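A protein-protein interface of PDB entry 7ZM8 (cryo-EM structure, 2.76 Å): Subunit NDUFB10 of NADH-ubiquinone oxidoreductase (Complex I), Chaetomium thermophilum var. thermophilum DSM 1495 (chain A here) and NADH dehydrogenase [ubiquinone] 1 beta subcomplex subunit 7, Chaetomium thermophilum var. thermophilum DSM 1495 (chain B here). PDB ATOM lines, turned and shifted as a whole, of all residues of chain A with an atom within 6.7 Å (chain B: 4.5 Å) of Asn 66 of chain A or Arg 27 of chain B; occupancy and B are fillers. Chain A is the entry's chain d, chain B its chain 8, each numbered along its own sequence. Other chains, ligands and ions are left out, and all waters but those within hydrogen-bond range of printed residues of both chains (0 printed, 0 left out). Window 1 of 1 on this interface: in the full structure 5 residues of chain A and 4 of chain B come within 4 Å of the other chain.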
ATOM      1  N   CYS A  59      18.980  -4.779 -16.083  1.00  0.00           N
ATOM      2  CA  CYS A  59      18.714  -5.667 -17.212  1.00  0.00           C
ATOM      3  C   CYS A  59      18.437  -7.081 -16.726  1.00  0.00           C
ATOM      4  O   CYS A  59      17.634  -7.805 -17.322  1.00  0.00           O
ATOM      5  CB  CYS A  59      19.897  -5.650 -18.185  1.00  0.00           C
ATOM      6  SG  CYS A  59      19.736  -6.643 -19.727  1.00  0.00           S
ATOM      7  N   ARG A  62      14.945  -7.121 -15.276  1.00  0.00           N
ATOM      8  CA  ARG A  62      14.000  -6.820 -16.335  1.00  0.00           C
ATOM      9  C   ARG A  62      13.793  -8.015 -17.253  1.00  0.00           C
ATOM     10  O   ARG A  62      12.665  -8.293 -17.670  1.00  0.00           O
ATOM     11  CB  ARG A  62      14.489  -5.607 -17.129  1.00  0.00           C
ATOM     12  CG  ARG A  62      13.729  -5.327 -18.397  1.00  0.00           C
ATOM     13  CD  ARG A  62      14.049  -3.951 -18.942  1.00  0.00           C
ATOM     14  NE  ARG A  62      15.485  -3.712 -19.074  1.00  0.00           N
ATOM     15  CZ  ARG A  62      16.163  -2.810 -18.369  1.00  0.00           C
ATOM     16  NH1 ARG A  62      17.463  -2.664 -18.557  1.00  0.00           N
ATOM     17  NH2 ARG A  62      15.545  -2.057 -17.473  1.00  0.00           N
ATOM     18  N   GLU A  63      14.861  -8.746 -17.551  1.00  0.00           N
ATOM     19  CA  GLU A  63      14.787  -9.842 -18.505  1.00  0.00           C
ATOM     20  C   GLU A  63      14.555 -11.184 -17.842  1.00  0.00           C
ATOM     21  O   GLU A  63      14.045 -12.103 -18.490  1.00  0.00           O
ATOM     22  CB  GLU A  63      16.069  -9.898 -19.341  1.00  0.00           C
ATOM     23  CG  GLU A  63      16.400  -8.640 -20.140  1.00  0.00           C
ATOM     24  CD  GLU A  63      15.202  -7.924 -20.754  1.00  0.00           C
ATOM     25  OE1 GLU A  63      15.333  -6.714 -21.027  1.00  0.00           O
ATOM     26  OE2 GLU A  63      14.168  -8.561 -21.049  1.00  0.00           O
ATOM     27  N   GLY A  64      14.913 -11.316 -16.570  1.00  0.00           N
ATOM     28  CA  GLY A  64      14.609 -12.512 -15.819  1.00  0.00           C
ATOM     29  C   GLY A  64      15.225 -13.772 -16.380  1.00  0.00           C
ATOM     30  O   GLY A  64      16.426 -14.005 -16.239  1.00  0.00           O
ATOM     31  N   VAL A  65      14.395 -14.609 -16.999  1.00  0.00           N
ATOM     32  CA  VAL A  65      14.873 -15.892 -17.494  1.00  0.00           C
ATOM     33  C   VAL A  65      15.820 -15.697 -18.673  1.00  0.00           C
ATOM     34  O   VAL A  65      16.908 -16.282 -18.719  1.00  0.00           O
ATOM     35  CB  VAL A  65      13.686 -16.806 -17.849  1.00  0.00           C
ATOM     36  CG1 VAL A  65      12.820 -16.213 -18.938  1.00  0.00           C
ATOM     37  CG2 VAL A  65      14.158 -18.171 -18.209  1.00  0.00           C
ATOM     38  N   ASN A  66      15.434 -14.871 -19.641  1.00  0.00           N
ATOM     39  CA  ASN A  66      16.284 -14.656 -20.806  1.00  0.00           C
ATOM     40  C   ASN A  66      17.155 -13.418 -20.650  1.00  0.00           C
ATOM     41  O   ASN A  66      17.233 -12.572 -21.530  1.00  0.00           O
ATOM     42  CB  ASN A  66      15.439 -14.588 -22.070  1.00  0.00           C
ATOM     43  CG  ASN A  66      14.173 -13.814 -21.882  1.00  0.00           C
ATOM     44  OD1 ASN A  66      14.179 -12.732 -21.307  1.00  0.00           O
ATOM     45  ND2 ASN A  66      13.070 -14.364 -22.358  1.00  0.00           N
ATOM     46  N   HIS A  67      17.935 -13.400 -19.582  1.00  0.00           N
ATOM     47  CA  HIS A  67      18.956 -12.348 -19.405  1.00  0.00           C
ATOM     48  C   HIS A  67      20.205 -12.880 -20.104  1.00  0.00           C
ATOM     49  O   HIS A  67      21.065 -12.078 -20.468  1.00  0.00           O
ATOM     50  CB  HIS A  67      19.224 -12.161 -17.904  1.00  0.00           C
ATOM     51  CG  HIS A  67      19.923 -13.307 -17.256  1.00  0.00           C
ATOM     52  ND1 HIS A  67      21.286 -13.314 -17.039  1.00  0.00           N
ATOM     53  CD2 HIS A  67      19.464 -14.485 -16.787  1.00  0.00           C
ATOM     54  CE1 HIS A  67      21.632 -14.446 -16.462  1.00  0.00           C
ATOM     55  NE2 HIS A  67      20.535 -15.180 -16.301  1.00  0.00           N
ATOM     56  N   LEU A  68      20.301 -14.205 -20.248  1.00  0.00           N
ATOM     57  CA  LEU A  68      21.469 -14.812 -20.862  1.00  0.00           C
ATOM     58  C   LEU A  68      21.576 -14.511 -22.349  1.00  0.00           C
ATOM     59  O   LEU A  68      22.604 -14.827 -22.954  1.00  0.00           O
ATOM     60  CB  LEU A  68      21.434 -16.318 -20.628  1.00  0.00           C
ATOM     61  CG  LEU A  68      22.059 -16.752 -19.305  1.00  0.00           C
ATOM     62  CD1 LEU A  68      21.938 -18.250 -19.093  1.00  0.00           C
ATOM     63  CD2 LEU A  68      23.498 -16.303 -19.249  1.00  0.00           C
ATOM     64  N   GLU A  69      20.544 -13.922 -22.950  1.00  0.00           N
ATOM     65  CA  GLU A  69      20.583 -13.529 -24.345  1.00  0.00           C
ATOM     66  C   GLU A  69      20.177 -12.083 -24.568  1.00  0.00           C
ATOM     67  O   GLU A  69      20.017 -11.677 -25.722  1.00  0.00           O
ATOM     68  CB  GLU A  69      19.691 -14.453 -25.184  1.00  0.00           C
ATOM     69  CG  GLU A  69      18.241 -14.478 -24.778  1.00  0.00           C
ATOM     70  CD  GLU A  69      17.378 -13.547 -25.603  1.00  0.00           C
ATOM     71  OE1 GLU A  69      17.812 -13.151 -26.705  1.00  0.00           O
ATOM     72  OE2 GLU A  69      16.257 -13.224 -25.157  1.00  0.00           O
ATOM     73  N   LYS A  70      20.011 -11.297 -23.507  1.00  0.00           N
ATOM     74  CA  LYS A  70      19.631  -9.901 -23.626  1.00  0.00           C
ATOM     75  C   LYS A  70      20.581  -8.938 -22.938  1.00  0.00           C
ATOM     76  O   LYS A  70      20.504  -7.735 -23.205  1.00  0.00           O
ATOM     77  CB  LYS A  70      18.222  -9.681 -23.057  1.00  0.00           C
ATOM     78  CG  LYS A  70      17.134 -10.450 -23.765  1.00  0.00           C
ATOM     79  CD  LYS A  70      17.023 -10.033 -25.213  1.00  0.00           C
ATOM     80  CE  LYS A  70      16.532  -8.600 -25.328  1.00  0.00           C
ATOM     81  NZ  LYS A  70      15.144  -8.453 -24.806  1.00  0.00           N
ATOM     82  N   CYS A  71      21.466  -9.421 -22.066  1.00  0.00           N
ATOM     83  CA  CYS A  71      22.319  -8.559 -21.259  1.00  0.00           C
ATOM     84  C   CYS A  71      23.799  -8.813 -21.532  1.00  0.00           C
ATOM     85  O   CYS A  71      24.642  -8.571 -20.670  1.00  0.00           O
ATOM     86  CB  CYS A  71      22.006  -8.735 -19.771  1.00  0.00           C
ATOM     87  SG  CYS A  71      20.267  -8.560 -19.288  1.00  0.00           S
ATOM     88  N   MET B  17       9.263 -18.232 -28.174  1.00  0.00           N
ATOM     89  CA  MET B  17       9.536 -18.837 -26.843  1.00  0.00           C
ATOM     90  C   MET B  17      10.253 -17.805 -25.968  1.00  0.00           C
ATOM     91  O   MET B  17       9.965 -17.762 -24.768  1.00  0.00           O
ATOM     92  CB  MET B  17      10.374 -20.103 -26.995  1.00  0.00           C
ATOM     93  CG  MET B  17       9.759 -21.090 -27.962  1.00  0.00           C
ATOM     94  SD  MET B  17      10.577 -22.699 -28.023  1.00  0.00           S
ATOM     95  CE  MET B  17      12.228 -22.235 -28.536  1.00  0.00           C
ATOM     96  N   ARG B  18      11.155 -17.011 -26.550  1.00  0.00           N
ATOM     97  CA  ARG B  18      11.841 -15.924 -25.806  1.00  0.00           C
ATOM     98  C   ARG B  18      10.830 -14.854 -25.442  1.00  0.00           C
ATOM     99  O   ARG B  18      10.882 -14.350 -24.315  1.00  0.00           O
ATOM    100  CB  ARG B  18      12.908 -15.276 -26.687  1.00  0.00           C
ATOM    101  CG  ARG B  18      13.269 -13.840 -26.349  1.00  0.00           C
ATOM    102  CD  ARG B  18      14.162 -13.311 -27.452  1.00  0.00           C
ATOM    103  NE  ARG B  18      13.485 -13.095 -28.721  1.00  0.00           N
ATOM    104  CZ  ARG B  18      13.123 -11.904 -29.179  1.00  0.00           C
ATOM    105  NH1 ARG B  18      12.510 -11.798 -30.345  1.00  0.00           N
ATOM    106  NH2 ARG B  18      13.377 -10.818 -28.470  1.00  0.00           N
ATOM    107  N   LYS B  21       8.551 -15.929 -22.511  1.00  0.00           N
ATOM    108  CA  LYS B  21       9.216 -16.253 -21.251  1.00  0.00           C
ATOM    109  C   LYS B  21       9.056 -17.726 -20.885  1.00  0.00           C
ATOM    110  O   LYS B  21       8.772 -18.070 -19.739  1.00  0.00           O
ATOM    111  CB  LYS B  21       8.701 -15.356 -20.124  1.00  0.00           C
ATOM    112  CG  LYS B  21       9.157 -13.902 -20.203  1.00  0.00           C
ATOM    113  CD  LYS B  21      10.358 -13.636 -19.309  1.00  0.00           C
ATOM    114  CE  LYS B  21      10.084 -14.093 -17.887  1.00  0.00           C
ATOM    115  NZ  LYS B  21      11.209 -13.787 -16.961  1.00  0.00           N
ATOM    116  N   VAL B  22       9.216 -18.604 -21.868  1.00  0.00           N
ATOM    117  CA  VAL B  22       9.193 -20.045 -21.588  1.00  0.00           C
ATOM    118  C   VAL B  22      10.458 -20.429 -20.832  1.00  0.00           C
ATOM    119  O   VAL B  22      11.537 -19.894 -21.136  1.00  0.00           O
ATOM    120  CB  VAL B  22       9.072 -20.838 -22.890  1.00  0.00           C
ATOM    121  CG1 VAL B  22       8.712 -22.282 -22.599  1.00  0.00           C
ATOM    122  CG2 VAL B  22       8.049 -20.214 -23.795  1.00  0.00           C
ATOM    123  N   PRO B  23      10.383 -21.310 -19.837  1.00  0.00           N
ATOM    124  CA  PRO B  23      11.611 -21.793 -19.194  1.00  0.00           C
ATOM    125  C   PRO B  23      12.501 -22.520 -20.192  1.00  0.00           C
ATOM    126  O   PRO B  23      12.019 -23.217 -21.084  1.00  0.00           O
ATOM    127  CB  PRO B  23      11.090 -22.733 -18.105  1.00  0.00           C
ATOM    128  CG  PRO B  23       9.717 -22.225 -17.809  1.00  0.00           C
ATOM    129  CD  PRO B  23       9.177 -21.765 -19.127  1.00  0.00           C
ATOM    130  N   LEU B  24      13.814 -22.349 -20.028  1.00  0.00           N
ATOM    131  CA  LEU B  24      14.761 -22.811 -21.042  1.00  0.00           C
ATOM    132  C   LEU B  24      14.679 -24.308 -21.277  1.00  0.00           C
ATOM    133  O   LEU B  24      14.739 -24.758 -22.427  1.00  0.00           O
ATOM    134  CB  LEU B  24      16.190 -22.414 -20.675  1.00  0.00           C
ATOM    135  CG  LEU B  24      16.654 -21.012 -21.052  1.00  0.00           C
ATOM    136  CD1 LEU B  24      16.634 -20.954 -22.547  1.00  0.00           C
ATOM    137  CD2 LEU B  24      15.781 -19.949 -20.532  1.00  0.00           C
ATOM    138  N   ALA B  25      14.562 -25.101 -20.214  1.00  0.00           N
ATOM    139  CA  ALA B  25      14.531 -26.547 -20.389  1.00  0.00           C
ATOM    140  C   ALA B  25      13.321 -27.004 -21.186  1.00  0.00           C
ATOM    141  O   ALA B  25      13.304 -28.138 -21.669  1.00  0.00           O
ATOM    142  CB  ALA B  25      14.553 -27.243 -19.032  1.00  0.00           C
ATOM    143  N   TYR B  26      12.315 -26.147 -21.341  1.00  0.00           N
ATOM    144  CA  TYR B  26      11.082 -26.496 -22.028  1.00  0.00           C
ATOM    145  C   TYR B  26      10.927 -25.758 -23.346  1.00  0.00           C
ATOM    146  O   TYR B  26       9.822 -25.676 -23.883  1.00  0.00           O
ATOM    147  CB  TYR B  26       9.893 -26.231 -21.110  1.00  0.00           C
ATOM    148  CG  TYR B  26       9.949 -27.096 -19.881  1.00  0.00           C
ATOM    149  CD1 TYR B  26      10.164 -28.463 -19.989  1.00  0.00           C
ATOM    150  CD2 TYR B  26       9.826 -26.548 -18.617  1.00  0.00           C
ATOM    151  CE1 TYR B  26      10.230 -29.260 -18.874  1.00  0.00           C
ATOM    152  CE2 TYR B  26       9.888 -27.339 -17.491  1.00  0.00           C
ATOM    153  CZ  TYR B  26      10.093 -28.693 -17.625  1.00  0.00           C
ATOM    154  OH  TYR B  26      10.157 -29.486 -16.504  1.00  0.00           O
ATOM    155  N   ARG B  27      12.018 -25.227 -23.882  1.00  0.00           N
ATOM    156  CA  ARG B  27      12.017 -24.622 -25.210  1.00  0.00           C
ATOM    157  C   ARG B  27      12.254 -25.676 -26.278  1.00  0.00           C
ATOM    158  O   ARG B  27      13.108 -25.553 -27.146  1.00  0.00           O
ATOM    159  CB  ARG B  27      13.058 -23.518 -25.267  1.00  0.00           C
ATOM    160  CG  ARG B  27      12.867 -22.516 -24.166  1.00  0.00           C
ATOM    161  CD  ARG B  27      13.255 -21.134 -24.564  1.00  0.00           C
ATOM    162  NE  ARG B  27      12.953 -20.219 -23.479  1.00  0.00           N
ATOM    163  CZ  ARG B  27      13.232 -18.927 -23.493  1.00  0.00           C
ATOM    164  NH1 ARG B  27      13.844 -18.394 -24.535  1.00  0.00           N
ATOM    165  NH2 ARG B  27      12.912 -18.175 -22.455  1.00  0.00           N
ATOM    166  N   ASP B  28      11.476 -26.743 -26.184  1.00  0.00           N
ATOM    167  CA  ASP B  28      11.542 -27.879 -27.076  1.00  0.00           C
ATOM    168  C   ASP B  28      10.380 -27.830 -28.064  1.00  0.00           C
ATOM    169  O   ASP B  28       9.637 -26.851 -28.129  1.00  0.00           O
ATOM    170  CB  ASP B  28      11.604 -29.169 -26.251  1.00  0.00           C
ATOM    171  CG  ASP B  28      10.370 -29.391 -25.393  1.00  0.00           C
ATOM    172  OD1 ASP B  28       9.460 -28.535 -25.385  1.00  0.00           O
ATOM    173  OD2 ASP B  28      10.318 -30.432 -24.706  1.00  0.00           O
ATOM    174  N   ALA B  31       6.736 -26.780 -27.117  1.00  0.00           N
ATOM    175  CA  ALA B  31       6.553 -25.551 -26.360  1.00  0.00           C
ATOM    176  C   ALA B  31       5.415 -24.692 -26.889  1.00  0.00           C
ATOM    177  O   ALA B  31       5.052 -23.709 -26.242  1.00  0.00           O
ATOM    178  CB  ALA B  31       7.850 -24.740 -26.350  1.00  0.00           C
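The backbone carbonyl oxygen (O) of Arg 18 of chain B is in hydrogen-bond range of the side-chain amide nitrogen (ND2) of Asn 66 of chain A, at 2.9 Å. NZ of Lys 21 of chain B lies close to N of Val 65 of chain A, 3.3 Å away.
Of the 11 printed residues of chain A, 5 touch a printed residue of chain B. Hydrophobic or aromatic side chains of chain A that line the printed part of chain B: Val 65. Of the 11 printed residues of chain B, 4 touch a printed residue of chain A. Among the printed residues, 7 pairs touch across the chains.
Of the printed residues of chain B, Gly 64 of chain A touches Lys 21. Of the printed residues of chain B, Val 65 of chain A touches Lys 21 and Leu 24. Asn 66 of chain A touches just these residues of chain B: Arg 18 (2.9 Å) and Arg 27 (3.8 Å). The nearest residue of chain B that does not touch Asn 66 of chain A is Lys 21 of chain B (4.1 Å). The nearest residue of chain A that does not touch Arg 27 of chain B is Val 65 of chain A (4.03 Å).
Glu 63 of chain A touches Lys 21 of chain B. Gly 64 of chain A touches Lys 21 of chain B. Val 65 of chain A touches Leu 24 of chain B. Arg 27 of chain B touches Asn 66 of chain A (NH2 to ND2, 3.8 Å). Glu 69 of chain A touches Arg 18 of chain B.
OE1 of Glu 63 of chain A lies within salt-bridge range of NE of Arg 62 of chain A. The backbone carbonyl oxygen (O) of Glu 63 of chain A lies close to the side-chain amide oxygen (OD1) of Asn 66 of chain A (2.9 Å). OE2 of Glu 63 of chain A is in salt-bridge range of NZ of Lys 70 of chain A (3.9 Å). The backbone carbonyl oxygen (O) of Val 22 of chain B sits at hydrogen-bond distance from the guanidinium group (NH2) of Arg 27 of chain B, 2.6 Å away. SG of Cys 59 of chain A is disulfide-bonded to SG of Cys 71 of chain A, 2.0 Å away.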
